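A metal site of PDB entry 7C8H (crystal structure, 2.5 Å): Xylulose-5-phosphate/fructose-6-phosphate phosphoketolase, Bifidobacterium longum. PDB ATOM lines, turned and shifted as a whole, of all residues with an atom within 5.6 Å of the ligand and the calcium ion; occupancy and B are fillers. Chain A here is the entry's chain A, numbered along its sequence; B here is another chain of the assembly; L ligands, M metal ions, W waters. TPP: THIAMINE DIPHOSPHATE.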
ATOM      1  N   GLY A  66     -25.273  24.237  17.203  1.00  0.00           N
ATOM      2  CA  GLY A  66     -26.439  23.424  16.762  1.00  0.00           C
ATOM      3  C   GLY A  66     -26.692  22.161  17.594  1.00  0.00           C
ATOM      4  O   GLY A  66     -27.800  21.998  18.142  1.00  0.00           O
ATOM      5  N   THR A  67     -25.695  21.281  17.649  1.00  0.00           N
ATOM      6  CA  THR A  67     -25.781  19.979  18.323  1.00  0.00           C
ATOM      7  C   THR A  67     -25.841  20.196  19.837  1.00  0.00           C
ATOM      8  O   THR A  67     -26.601  19.468  20.496  1.00  0.00           O
ATOM      9  CB  THR A  67     -24.633  19.073  17.854  1.00  0.00           C
ATOM     10  OG1 THR A  67     -24.978  17.771  18.308  1.00  0.00           O
ATOM     11  CG2 THR A  67     -23.283  19.469  18.391  1.00  0.00           C
ATOM     12  N   PRO A  95     -21.546  13.464  17.900  1.00  0.00           N
ATOM     13  CA  PRO A  95     -21.369  14.838  17.474  1.00  0.00           C
ATOM     14  C   PRO A  95     -20.237  15.503  18.274  1.00  0.00           C
ATOM     15  O   PRO A  95     -20.466  16.382  19.091  1.00  0.00           O
ATOM     16  CB  PRO A  95     -22.736  15.503  17.700  1.00  0.00           C
ATOM     17  CG  PRO A  95     -23.684  14.368  18.023  1.00  0.00           C
ATOM     18  CD  PRO A  95     -22.835  13.252  18.575  1.00  0.00           C
ATOM     19  N   HIS A  97     -18.085  17.603  17.628  1.00  0.00           N
ATOM     20  CA  HIS A  97     -18.027  19.072  17.418  1.00  0.00           C
ATOM     21  C   HIS A  97     -18.852  19.778  18.511  1.00  0.00           C
ATOM     22  O   HIS A  97     -18.634  20.994  18.715  1.00  0.00           O
ATOM     23  CB  HIS A  97     -18.388  19.407  15.953  1.00  0.00           C
ATOM     24  CG  HIS A  97     -19.721  18.876  15.517  1.00  0.00           C
ATOM     25  ND1 HIS A  97     -19.906  17.563  15.074  1.00  0.00           N
ATOM     26  CD2 HIS A  97     -20.933  19.486  15.432  1.00  0.00           C
ATOM     27  CE1 HIS A  97     -21.174  17.389  14.777  1.00  0.00           C
ATOM     28  NE2 HIS A  97     -21.813  18.556  14.972  1.00  0.00           N
ATOM     29  N   GLY A 154     -14.883  12.445  18.167  1.00  0.00           N
ATOM     30  CA  GLY A 154     -16.009  12.715  17.259  1.00  0.00           C
ATOM     31  C   GLY A 154     -15.677  13.738  16.189  1.00  0.00           C
ATOM     32  O   GLY A 154     -16.641  14.447  15.700  1.00  0.00           O
ATOM     33  N   GLY A 155     -14.387  13.817  15.806  1.00  0.00           N
ATOM     34  CA  GLY A 155     -13.883  14.756  14.789  1.00  0.00           C
ATOM     35  C   GLY A 155     -14.170  14.190  13.429  1.00  0.00           C
ATOM     36  O   GLY A 155     -14.871  14.823  12.621  1.00  0.00           O
ATOM     37  N   GLU A 156     -13.662  12.994  13.167  1.00  0.00           N
ATOM     38  CA  GLU A 156     -14.035  12.244  11.966  1.00  0.00           C
ATOM     39  C   GLU A 156     -15.252  11.426  12.364  1.00  0.00           C
ATOM     40  O   GLU A 156     -15.082  10.504  13.189  1.00  0.00           O
ATOM     41  CB  GLU A 156     -12.872  11.406  11.472  1.00  0.00           C
ATOM     42  CG  GLU A 156     -13.095  10.843  10.077  1.00  0.00           C
ATOM     43  CD  GLU A 156     -11.848  10.122   9.602  1.00  0.00           C
ATOM     44  OE1 GLU A 156     -10.801  10.795   9.511  1.00  0.00           O
ATOM     45  OE2 GLU A 156     -11.912   8.882   9.442  1.00  0.00           O
ATOM     46  N   LEU A 157     -16.414  11.791  11.819  1.00  0.00           N
ATOM     47  CA  LEU A 157     -17.726  11.174  12.121  1.00  0.00           C
ATOM     48  C   LEU A 157     -17.749   9.737  11.614  1.00  0.00           C
ATOM     49  O   LEU A 157     -17.182   9.489  10.551  1.00  0.00           O
ATOM     50  CB  LEU A 157     -18.822  11.988  11.459  1.00  0.00           C
ATOM     51  CG  LEU A 157     -19.040  13.365  12.084  1.00  0.00           C
ATOM     52  CD1 LEU A 157     -20.175  14.087  11.376  1.00  0.00           C
ATOM     53  CD2 LEU A 157     -19.312  13.255  13.579  1.00  0.00           C
ATOM     54  N   TYR A 159     -17.758   6.689  13.992  1.00  0.00           N
ATOM     55  CA  TYR A 159     -17.188   5.610  14.850  1.00  0.00           C
ATOM     56  C   TYR A 159     -17.900   5.587  16.197  1.00  0.00           C
ATOM     57  O   TYR A 159     -17.414   4.941  17.145  1.00  0.00           O
ATOM     58  CB  TYR A 159     -15.676   5.806  14.940  1.00  0.00           C
ATOM     59  CG  TYR A 159     -15.097   6.160  13.596  1.00  0.00           C
ATOM     60  CD1 TYR A 159     -15.343   5.389  12.477  1.00  0.00           C
ATOM     61  CD2 TYR A 159     -14.352   7.299  13.433  1.00  0.00           C
ATOM     62  CE1 TYR A 159     -14.871   5.746  11.231  1.00  0.00           C
ATOM     63  CE2 TYR A 159     -13.873   7.678  12.188  1.00  0.00           C
ATOM     64  CZ  TYR A 159     -14.133   6.907  11.073  1.00  0.00           C
ATOM     65  OH  TYR A 159     -13.661   7.310   9.864  1.00  0.00           O
ATOM     66  N   GLY A 181     -25.035  11.458  15.757  1.00  0.00           N
ATOM     67  CA  GLY A 181     -25.571  12.516  14.888  1.00  0.00           C
ATOM     68  C   GLY A 181     -26.428  11.931  13.768  1.00  0.00           C
ATOM     69  O   GLY A 181     -26.130  10.815  13.316  1.00  0.00           O
ATOM     70  N   ASP A 182     -27.477  12.633  13.348  1.00  0.00           N
ATOM     71  CA  ASP A 182     -28.365  12.142  12.279  1.00  0.00           C
ATOM     72  C   ASP A 182     -27.633  12.271  10.932  1.00  0.00           C
ATOM     73  O   ASP A 182     -27.892  11.437  10.076  1.00  0.00           O
ATOM     74  CB  ASP A 182     -29.784  12.747  12.374  1.00  0.00           C
ATOM     75  CG  ASP A 182     -29.893  14.256  12.321  1.00  0.00           C
ATOM     76  OD1 ASP A 182     -28.897  14.894  12.548  1.00  0.00           O
ATOM     77  OD2 ASP A 182     -31.014  14.774  12.057  1.00  0.00           O
ATOM     78  N   GLY A 183     -26.718  13.228  10.777  1.00  0.00           N
ATOM     79  CA  GLY A 183     -25.736  13.312   9.667  1.00  0.00           C
ATOM     80  C   GLY A 183     -24.650  12.233   9.756  1.00  0.00           C
ATOM     81  O   GLY A 183     -24.401  11.543   8.744  1.00  0.00           O
ATOM     82  N   GLU A 184     -24.019  12.068  10.915  1.00  0.00           N
ATOM     83  CA  GLU A 184     -23.091  10.949  11.169  1.00  0.00           C
ATOM     84  C   GLU A 184     -23.769   9.633  10.723  1.00  0.00           C
ATOM     85  O   GLU A 184     -23.075   8.790  10.138  1.00  0.00           O
ATOM     86  CB  GLU A 184     -22.672  10.925  12.644  1.00  0.00           C
ATOM     87  CG  GLU A 184     -21.751   9.778  12.999  1.00  0.00           C
ATOM     88  CD  GLU A 184     -21.255   9.787  14.430  1.00  0.00           C
ATOM     89  OE1 GLU A 184     -21.946  10.355  15.308  1.00  0.00           O
ATOM     90  OE2 GLU A 184     -20.190   9.223  14.670  1.00  0.00           O
ATOM     91  N   ALA A 185     -25.080   9.477  10.946  1.00  0.00           N
ATOM     92  CA  ALA A 185     -25.830   8.242  10.600  1.00  0.00           C
ATOM     93  C   ALA A 185     -25.747   7.931   9.089  1.00  0.00           C
ATOM     94  O   ALA A 185     -25.990   6.767   8.711  1.00  0.00           O
ATOM     95  CB  ALA A 185     -27.247   8.351  11.039  1.00  0.00           C
ATOM     96  N   THR A 187     -22.912   8.200   7.297  1.00  0.00           N
ATOM     97  CA  THR A 187     -21.569   7.650   6.968  1.00  0.00           C
ATOM     98  C   THR A 187     -21.756   6.144   6.892  1.00  0.00           C
ATOM     99  O   THR A 187     -22.733   5.656   7.499  1.00  0.00           O
ATOM    100  CB  THR A 187     -20.491   7.963   8.000  1.00  0.00           C
ATOM    101  OG1 THR A 187     -20.878   7.409   9.261  1.00  0.00           O
ATOM    102  CG2 THR A 187     -20.248   9.437   8.194  1.00  0.00           C
ATOM    103  N   HIS A 213     -29.467  11.628  17.743  1.00  0.00           N
ATOM    104  CA  HIS A 213     -29.623  13.096  17.840  1.00  0.00           C
ATOM    105  C   HIS A 213     -30.294  13.572  16.548  1.00  0.00           C
ATOM    106  O   HIS A 213     -29.629  14.177  15.655  1.00  0.00           O
ATOM    107  CB  HIS A 213     -28.258  13.673  18.193  1.00  0.00           C
ATOM    108  CG  HIS A 213     -28.294  15.092  18.628  1.00  0.00           C
ATOM    109  ND1 HIS A 213     -29.460  15.734  18.940  1.00  0.00           N
ATOM    110  CD2 HIS A 213     -27.291  15.977  18.826  1.00  0.00           C
ATOM    111  CE1 HIS A 213     -29.188  16.965  19.289  1.00  0.00           C
ATOM    112  NE2 HIS A 213     -27.848  17.124  19.258  1.00  0.00           N
ATOM    113  N   ASN A 215     -31.796  15.893  14.999  1.00  0.00           N
ATOM    114  CA  ASN A 215     -32.067  17.343  15.036  1.00  0.00           C
ATOM    115  C   ASN A 215     -32.325  17.849  13.613  1.00  0.00           C
ATOM    116  O   ASN A 215     -32.365  19.048  13.408  1.00  0.00           O
ATOM    117  CB  ASN A 215     -30.965  18.078  15.801  1.00  0.00           C
ATOM    118  CG  ASN A 215     -29.632  17.946  15.120  1.00  0.00           C
ATOM    119  OD1 ASN A 215     -29.585  17.574  13.960  1.00  0.00           O
ATOM    120  ND2 ASN A 215     -28.559  18.224  15.837  1.00  0.00           N
ATOM    121  N   GLY A 216     -32.502  16.950  12.637  1.00  0.00           N
ATOM    122  CA  GLY A 216     -33.107  17.289  11.342  1.00  0.00           C
ATOM    123  C   GLY A 216     -32.105  17.756  10.301  1.00  0.00           C
ATOM    124  O   GLY A 216     -32.494  17.833   9.117  1.00  0.00           O
ATOM    125  N   TYR A 217     -30.867  18.082  10.689  1.00  0.00           N
ATOM    126  CA  TYR A 217     -29.913  18.825   9.833  1.00  0.00           C
ATOM    127  C   TYR A 217     -28.515  18.390  10.170  1.00  0.00           C
ATOM    128  O   TYR A 217     -28.275  17.846  11.250  1.00  0.00           O
ATOM    129  CB  TYR A 217     -30.079  20.348   9.950  1.00  0.00           C
ATOM    130  CG  TYR A 217     -31.450  20.807   9.537  1.00  0.00           C
ATOM    131  CD1 TYR A 217     -31.781  20.924   8.201  1.00  0.00           C
ATOM    132  CD2 TYR A 217     -32.458  20.946  10.478  1.00  0.00           C
ATOM    133  CE1 TYR A 217     -33.071  21.248   7.823  1.00  0.00           C
ATOM    134  CE2 TYR A 217     -33.759  21.268  10.113  1.00  0.00           C
ATOM    135  CZ  TYR A 217     -34.061  21.413   8.774  1.00  0.00           C
ATOM    136  OH  TYR A 217     -35.326  21.741   8.412  1.00  0.00           O
ATOM    137  N   LYS A 218     -27.668  18.520   9.169  1.00  0.00           N
ATOM    138  CA  LYS A 218     -26.213  18.358   9.222  1.00  0.00           C
ATOM    139  C   LYS A 218     -25.708  19.770   8.934  1.00  0.00           C
ATOM    140  O   LYS A 218     -26.348  20.698   9.467  1.00  0.00           O
ATOM    141  CB  LYS A 218     -25.749  17.207   8.314  1.00  0.00           C
ATOM    142  CG  LYS A 218     -26.405  17.051   6.939  1.00  0.00           C
ATOM    143  CD  LYS A 218     -25.870  15.856   6.185  1.00  0.00           C
ATOM    144  CE  LYS A 218     -26.350  15.733   4.755  1.00  0.00           C
ATOM    145  NZ  LYS A 218     -27.664  15.056   4.656  1.00  0.00           N
ATOM    146  N   ILE A 219     -24.655  19.967   8.144  1.00  0.00           N
ATOM    147  CA  ILE A 219     -24.081  21.333   7.969  1.00  0.00           C
ATOM    148  C   ILE A 219     -25.086  22.220   7.234  1.00  0.00           C
ATOM    149  O   ILE A 219     -25.429  23.290   7.772  1.00  0.00           O
ATOM    150  CB  ILE A 219     -22.749  21.311   7.220  1.00  0.00           C
ATOM    151  CG1 ILE A 219     -21.674  20.544   8.008  1.00  0.00           C
ATOM    152  CG2 ILE A 219     -22.337  22.746   6.935  1.00  0.00           C
ATOM    153  CD1 ILE A 219     -20.474  20.179   7.178  1.00  0.00           C
ATOM    154  N   THR A 223     -31.190  15.924   7.023  1.00  0.00           N
ATOM    155  CA  THR A 223     -30.632  14.578   7.111  1.00  0.00           C
ATOM    156  C   THR A 223     -31.660  13.631   6.537  1.00  0.00           C
ATOM    157  O   THR A 223     -32.862  13.833   6.775  1.00  0.00           O
ATOM    158  CB  THR A 223     -30.275  14.260   8.559  1.00  0.00           C
ATOM    159  OG1 THR A 223     -31.421  14.595   9.340  1.00  0.00           O
ATOM    160  CG2 THR A 223     -29.030  15.007   8.993  1.00  0.00           C
ATOM    161  N   LYS A 300     -32.655  21.613  15.811  1.00  0.00           N
ATOM    162  CA  LYS A 300     -31.203  21.874  15.799  1.00  0.00           C
ATOM    163  C   LYS A 300     -31.012  23.310  16.278  1.00  0.00           C
ATOM    164  O   LYS A 300     -31.755  24.170  15.801  1.00  0.00           O
ATOM    165  CB  LYS A 300     -30.570  21.689  14.419  1.00  0.00           C
ATOM    166  CG  LYS A 300     -29.048  21.810  14.424  1.00  0.00           C
ATOM    167  CD  LYS A 300     -28.305  21.017  13.348  1.00  0.00           C
ATOM    168  CE  LYS A 300     -26.820  21.221  13.383  1.00  0.00           C
ATOM    169  NZ  LYS A 300     -26.095  20.410  12.391  1.00  0.00           N
ATOM    170  N   HIS A 320     -25.816  25.424  12.795  1.00  0.00           N
ATOM    171  CA  HIS A 320     -24.904  24.269  12.944  1.00  0.00           C
ATOM    172  C   HIS A 320     -23.581  24.740  13.560  1.00  0.00           C
ATOM    173  O   HIS A 320     -23.086  24.072  14.513  1.00  0.00           O
ATOM    174  CB  HIS A 320     -24.704  23.545  11.618  1.00  0.00           C
ATOM    175  CG  HIS A 320     -23.519  22.658  11.639  1.00  0.00           C
ATOM    176  ND1 HIS A 320     -23.549  21.438  12.271  1.00  0.00           N
ATOM    177  CD2 HIS A 320     -22.267  22.823  11.152  1.00  0.00           C
ATOM    178  CE1 HIS A 320     -22.348  20.880  12.180  1.00  0.00           C
ATOM    179  NE2 HIS A 320     -21.558  21.701  11.466  1.00  0.00           N
ATOM    180  N   PRO B 435     -19.882  15.576   0.375  1.00  0.00           N
ATOM    181  CA  PRO B 435     -20.356  15.024   1.636  1.00  0.00           C
ATOM    182  C   PRO B 435     -20.874  16.117   2.559  1.00  0.00           C
ATOM    183  O   PRO B 435     -20.265  16.330   3.568  1.00  0.00           O
ATOM    184  CB  PRO B 435     -19.103  14.373   2.224  1.00  0.00           C
ATOM    185  CG  PRO B 435     -18.044  14.541   1.170  1.00  0.00           C
ATOM    186  CD  PRO B 435     -18.439  15.762   0.386  1.00  0.00           C
ATOM    187  N   ASP B 436     -21.951  16.805   2.143  1.00  0.00           N
ATOM    188  CA  ASP B 436     -22.583  17.940   2.880  1.00  0.00           C
ATOM    189  C   ASP B 436     -21.605  19.119   2.918  1.00  0.00           C
ATOM    190  O   ASP B 436     -21.647  19.881   3.883  1.00  0.00           O
ATOM    191  CB  ASP B 436     -23.059  17.457   4.265  1.00  0.00           C
ATOM    192  CG  ASP B 436     -23.842  18.454   5.099  1.00  0.00           C
ATOM    193  OD1 ASP B 436     -24.611  19.315   4.514  1.00  0.00           O
ATOM    194  OD2 ASP B 436     -23.687  18.362   6.334  1.00  0.00           O
ATOM    195  N   GLU B 437     -20.738  19.242   1.912  1.00  0.00           N
ATOM    196  CA  GLU B 437     -19.597  20.185   1.921  1.00  0.00           C
ATOM    197  C   GLU B 437     -19.541  21.026   0.651  1.00  0.00           C
ATOM    198  O   GLU B 437     -18.559  21.805   0.528  1.00  0.00           O
ATOM    199  CB  GLU B 437     -18.291  19.403   2.096  1.00  0.00           C
ATOM    200  CG  GLU B 437     -18.113  18.804   3.482  1.00  0.00           C
ATOM    201  CD  GLU B 437     -16.937  17.846   3.558  1.00  0.00           C
ATOM    202  OE1 GLU B 437     -16.048  17.961   2.711  1.00  0.00           O
ATOM    203  OE2 GLU B 437     -16.931  16.965   4.426  1.00  0.00           O
ATOM    204  N   LEU B 477     -23.828  12.644   3.782  1.00  0.00           N
ATOM    205  CA  LEU B 477     -22.597  12.702   4.620  1.00  0.00           C
ATOM    206  C   LEU B 477     -21.934  11.325   4.556  1.00  0.00           C
ATOM    207  O   LEU B 477     -22.054  10.520   5.515  1.00  0.00           O
ATOM    208  CB  LEU B 477     -22.938  13.206   6.020  1.00  0.00           C
ATOM    209  CG  LEU B 477     -21.843  13.306   7.090  1.00  0.00           C
ATOM    210  CD1 LEU B 477     -20.427  13.389   6.555  1.00  0.00           C
ATOM    211  CD2 LEU B 477     -22.146  14.481   8.007  1.00  0.00           C
ATOM    212  N   GLU B 479     -18.303  10.133   2.296  1.00  0.00           N
ATOM    213  CA  GLU B 479     -17.207  10.128   1.303  1.00  0.00           C
ATOM    214  C   GLU B 479     -17.345   8.873   0.423  1.00  0.00           C
ATOM    215  O   GLU B 479     -17.123   8.974  -0.782  1.00  0.00           O
ATOM    216  CB  GLU B 479     -15.875  10.205   2.037  1.00  0.00           C
ATOM    217  CG  GLU B 479     -15.671  11.508   2.764  1.00  0.00           C
ATOM    218  CD  GLU B 479     -16.336  11.681   4.129  1.00  0.00           C
ATOM    219  OE1 GLU B 479     -16.802  10.654   4.731  1.00  0.00           O
ATOM    220  OE2 GLU B 479     -16.394  12.855   4.586  1.00  0.00           O
ATOM    221  N   TYR B 501     -13.281  18.095   2.354  1.00  0.00           N
ATOM    222  CA  TYR B 501     -12.263  18.494   3.349  1.00  0.00           C
ATOM    223  C   TYR B 501     -11.115  17.514   3.170  1.00  0.00           C
ATOM    224  O   TYR B 501     -11.330  16.289   3.077  1.00  0.00           O
ATOM    225  CB  TYR B 501     -12.804  18.448   4.779  1.00  0.00           C
ATOM    226  CG  TYR B 501     -13.989  19.335   5.078  1.00  0.00           C
ATOM    227  CD1 TYR B 501     -14.445  20.312   4.211  1.00  0.00           C
ATOM    228  CD2 TYR B 501     -14.643  19.200   6.293  1.00  0.00           C
ATOM    229  CE1 TYR B 501     -15.513  21.127   4.546  1.00  0.00           C
ATOM    230  CE2 TYR B 501     -15.726  19.986   6.628  1.00  0.00           C
ATOM    231  CZ  TYR B 501     -16.161  20.971   5.757  1.00  0.00           C
ATOM    232  OH  TYR B 501     -17.236  21.726   6.158  1.00  0.00           O
ATOM    233  N   PHE B 504     -10.577  14.245   5.393  1.00  0.00           N
ATOM    234  CA  PHE B 504     -11.576  13.151   5.268  1.00  0.00           C
ATOM    235  C   PHE B 504     -11.524  12.443   3.894  1.00  0.00           C
ATOM    236  O   PHE B 504     -12.232  11.395   3.741  1.00  0.00           O
ATOM    237  CB  PHE B 504     -12.958  13.699   5.616  1.00  0.00           C
ATOM    238  CG  PHE B 504     -12.985  14.298   6.999  1.00  0.00           C
ATOM    239  CD1 PHE B 504     -12.304  13.705   8.045  1.00  0.00           C
ATOM    240  CD2 PHE B 504     -13.665  15.481   7.236  1.00  0.00           C
ATOM    241  CE1 PHE B 504     -12.295  14.285   9.294  1.00  0.00           C
ATOM    242  CE2 PHE B 504     -13.655  16.046   8.493  1.00  0.00           C
ATOM    243  CZ  PHE B 504     -12.978  15.441   9.518  1.00  0.00           C
ATOM    244  N   VAL B 507     -10.834   8.865   4.270  1.00  0.00           N
ATOM    245  CA  VAL B 507     -11.963   7.894   4.409  1.00  0.00           C
ATOM    246  C   VAL B 507     -12.050   7.009   3.156  1.00  0.00           C
ATOM    247  O   VAL B 507     -12.325   5.808   3.277  1.00  0.00           O
ATOM    248  CB  VAL B 507     -13.286   8.606   4.705  1.00  0.00           C
ATOM    249  CG1 VAL B 507     -14.484   7.676   4.503  1.00  0.00           C
ATOM    250  CG2 VAL B 507     -13.284   9.150   6.116  1.00  0.00           C
ATOM    251  N   HIS B 553      -8.791  17.352  11.925  1.00  0.00           N
ATOM    252  CA  HIS B 553      -9.078  17.805  10.532  1.00  0.00           C
ATOM    253  C   HIS B 553      -7.759  18.108   9.801  1.00  0.00           C
ATOM    254  O   HIS B 553      -7.827  18.605   8.676  1.00  0.00           O
ATOM    255  CB  HIS B 553     -10.029  19.014  10.565  1.00  0.00           C
ATOM    256  CG  HIS B 553     -11.431  18.662  10.925  1.00  0.00           C
ATOM    257  ND1 HIS B 553     -11.745  17.925  12.051  1.00  0.00           N
ATOM    258  CD2 HIS B 553     -12.605  18.978  10.324  1.00  0.00           C
ATOM    259  CE1 HIS B 553     -13.053  17.767  12.128  1.00  0.00           C
ATOM    260  NE2 HIS B 553     -13.614  18.408  11.072  1.00  0.00           N
HETATM  261  N1' TPP L   1     -16.945  13.695   6.805  1.00  0.00           N
HETATM  262  C2' TPP L   1     -16.471  13.101   7.898  1.00  0.00           C
HETATM  263  CM2 TPP L   1     -16.111  11.656   7.810  1.00  0.00           C
HETATM  264  N3' TPP L   1     -16.317  13.686   9.083  1.00  0.00           N
HETATM  265  C4' TPP L   1     -16.621  14.989   9.159  1.00  0.00           C
HETATM  266  N4' TPP L   1     -16.399  15.575  10.330  1.00  0.00           N
HETATM  267  C5' TPP L   1     -17.148  15.692   8.063  1.00  0.00           C
HETATM  268  C6' TPP L   1     -17.289  14.983   6.898  1.00  0.00           C
HETATM  269  C7' TPP L   1     -17.545  17.132   8.148  1.00  0.00           C
HETATM  270  N3  TPP L   1     -18.654  17.330   9.088  1.00  0.00           N
HETATM  271  C2  TPP L   1     -18.441  17.666  10.371  1.00  0.00           C
HETATM  272  S1  TPP L   1     -19.926  18.031  11.192  1.00  0.00           S
HETATM  273  C5  TPP L   1     -20.800  17.580   9.773  1.00  0.00           C
HETATM  274  C4  TPP L   1     -19.983  17.310   8.723  1.00  0.00           C
HETATM  275  CM4 TPP L   1     -20.365  17.048   7.303  1.00  0.00           C
HETATM  276  C6  TPP L   1     -22.287  17.489   9.858  1.00  0.00           C
HETATM  277  C7  TPP L   1     -22.679  16.588  10.990  1.00  0.00           C
HETATM  278  O7  TPP L   1     -24.096  16.652  11.235  1.00  0.00           O
HETATM  279  PA  TPP L   1     -24.700  15.694  12.355  1.00  0.00           P
HETATM  280  O1A TPP L   1     -26.133  15.610  12.004  1.00  0.00           O
HETATM  281  O2A TPP L   1     -24.015  14.396  12.649  1.00  0.00           O
HETATM  282  O3A TPP L   1     -24.429  16.690  13.593  1.00  0.00           O
HETATM  283  PB  TPP L   1     -25.243  17.843  14.394  1.00  0.00           P
HETATM  284  O1B TPP L   1     -25.495  17.158  15.699  1.00  0.00           O
HETATM  285  O2B TPP L   1     -26.533  18.241  13.727  1.00  0.00           O
HETATM  286  O3B TPP L   1     -24.319  19.021  14.444  1.00  0.00           O
HETATM  287 CA    CA M   1     -27.669  16.635  13.137  1.00  0.00          CA
HETATM  288  O   HOH W   1     -23.868  21.568  15.373  1.00  0.00           O
HETATM  289  O   HOH W   2     -27.287  15.458  15.120  1.00  0.00           O
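Water W2 lies within hydrogen-bond range of O1B of the ligand (2.5 Å), O of His 213 (2.7 Å), ND2 of Asn 215 (3.1 Å) and N of Asp 182 (3.3 Å).
Water W1 lies within hydrogen-bond range of an oxygen (O3B) of the ligand (2.7 Å), the backbone carbonyl oxygen of His 320 (2.8 Å) and the backbone NH of Thr 67 (2.9 Å).
Three residues have an atom within 4 Å of the calcium ion: Asp 182, Asn 215 and Tyr 217.
The nearest printed residue that does not touch the calcium ion is His 213 (4.03 Å).
Residues that only touch the ligand: Ile 219 (3.1 Å), Glu 437 of chain B (3.2 Å), Leu 477 of chain B (3.2 Å), Phe 504 of chain B (3.2 Å), Gly 181 (3.3 Å), Lys 218 (3.4 Å), Asp 436 of chain B (3.7 Å), Tyr 501 of chain B (3.7 Å), Pro 95 (3.8 Å), His 213 (3.8 Å), Pro 435 of chain B (3.8 Å) and Glu 156 (3.9 Å).
Of the 33 residues printed, 24 come within 4 Å of the ligand.
An oxygen (O2B) of the ligand binds the calcium ion (2.1 Å).
An oxygen (O1A) of the ligand binds the calcium ion.
The side-chain carboxylate (OD1) of Asp 182 is bound to the calcium ion (2.2 Å).
OD1 of Asn 215 is bound to the calcium ion, at 2.3 Å.
O of Tyr 217 is bound to the calcium ion (2.3 Å).
The calcium ion is bound by water W2.
The side-chain carboxylate (OD2) of Asp 182 is in hydrogen-bond range of the side-chain hydroxyl (OG1) of Thr 223 (2.8 Å).
The side-chain amino group of Lys 300 sits at hydrogen-bond distance from a ring nitrogen (ND1) of His 320, at 2.7 Å.
A ring nitrogen (NE2) of His 213 is in hydrogen-bond range of the backbone carbonyl oxygen of Thr 67, 2.9 Å away.
The backbone carbonyl oxygen (O) of Glu 184 lies within hydrogen-bond range of the side-chain hydroxyl (OG1) of Thr 187, at 2.7 Å.
OD2 of Asp 436 of chain B lies within hydrogen-bond range of N of Ile 219 (2.6 Å).
OE1 of Glu 437 of chain B sits at hydrogen-bond distance from N of Tyr 501 of chain B.
The backbone carbonyl oxygen of Leu 477 of chain B is in hydrogen-bond range of the backbone NH of Thr 187.
The backbone carbonyl oxygen (O) of His 320 sits at hydrogen-bond distance from the backbone NH (N) of Gly 66.
OE2 of Glu 479 of chain B sits at hydrogen-bond distance from N1' of the ligand, 2.4 Å away.
NZ of Lys 300 lies within salt-bridge range of O3B of the ligand.
O3B of the ligand sits at hydrogen-bond distance from NE2 of His 97.
An oxygen (O1B) of the ligand is in hydrogen-bond range of the side-chain hydroxyl of Thr 67 (2.7 Å).
The backbone NH (N) of Gly 183 is in hydrogen-bond range of an oxygen (O2A) of the ligand.
A nitrogen (N4') of the ligand sits at hydrogen-bond distance from the backbone carbonyl oxygen (O) of Gly 155 (2.9 Å).
An oxygen (O2A) of the ligand is in hydrogen-bond range of the backbone NH (N) of Glu 184, at 2.9 Å.
The backbone NH (N) of Leu 157 is in hydrogen-bond range of a nitrogen (N3') of the ligand (3.3 Å).
A ring nitrogen (ND1) of His 320 lies within hydrogen-bond range of an oxygen (O3B) of the ligand (3.3 Å).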
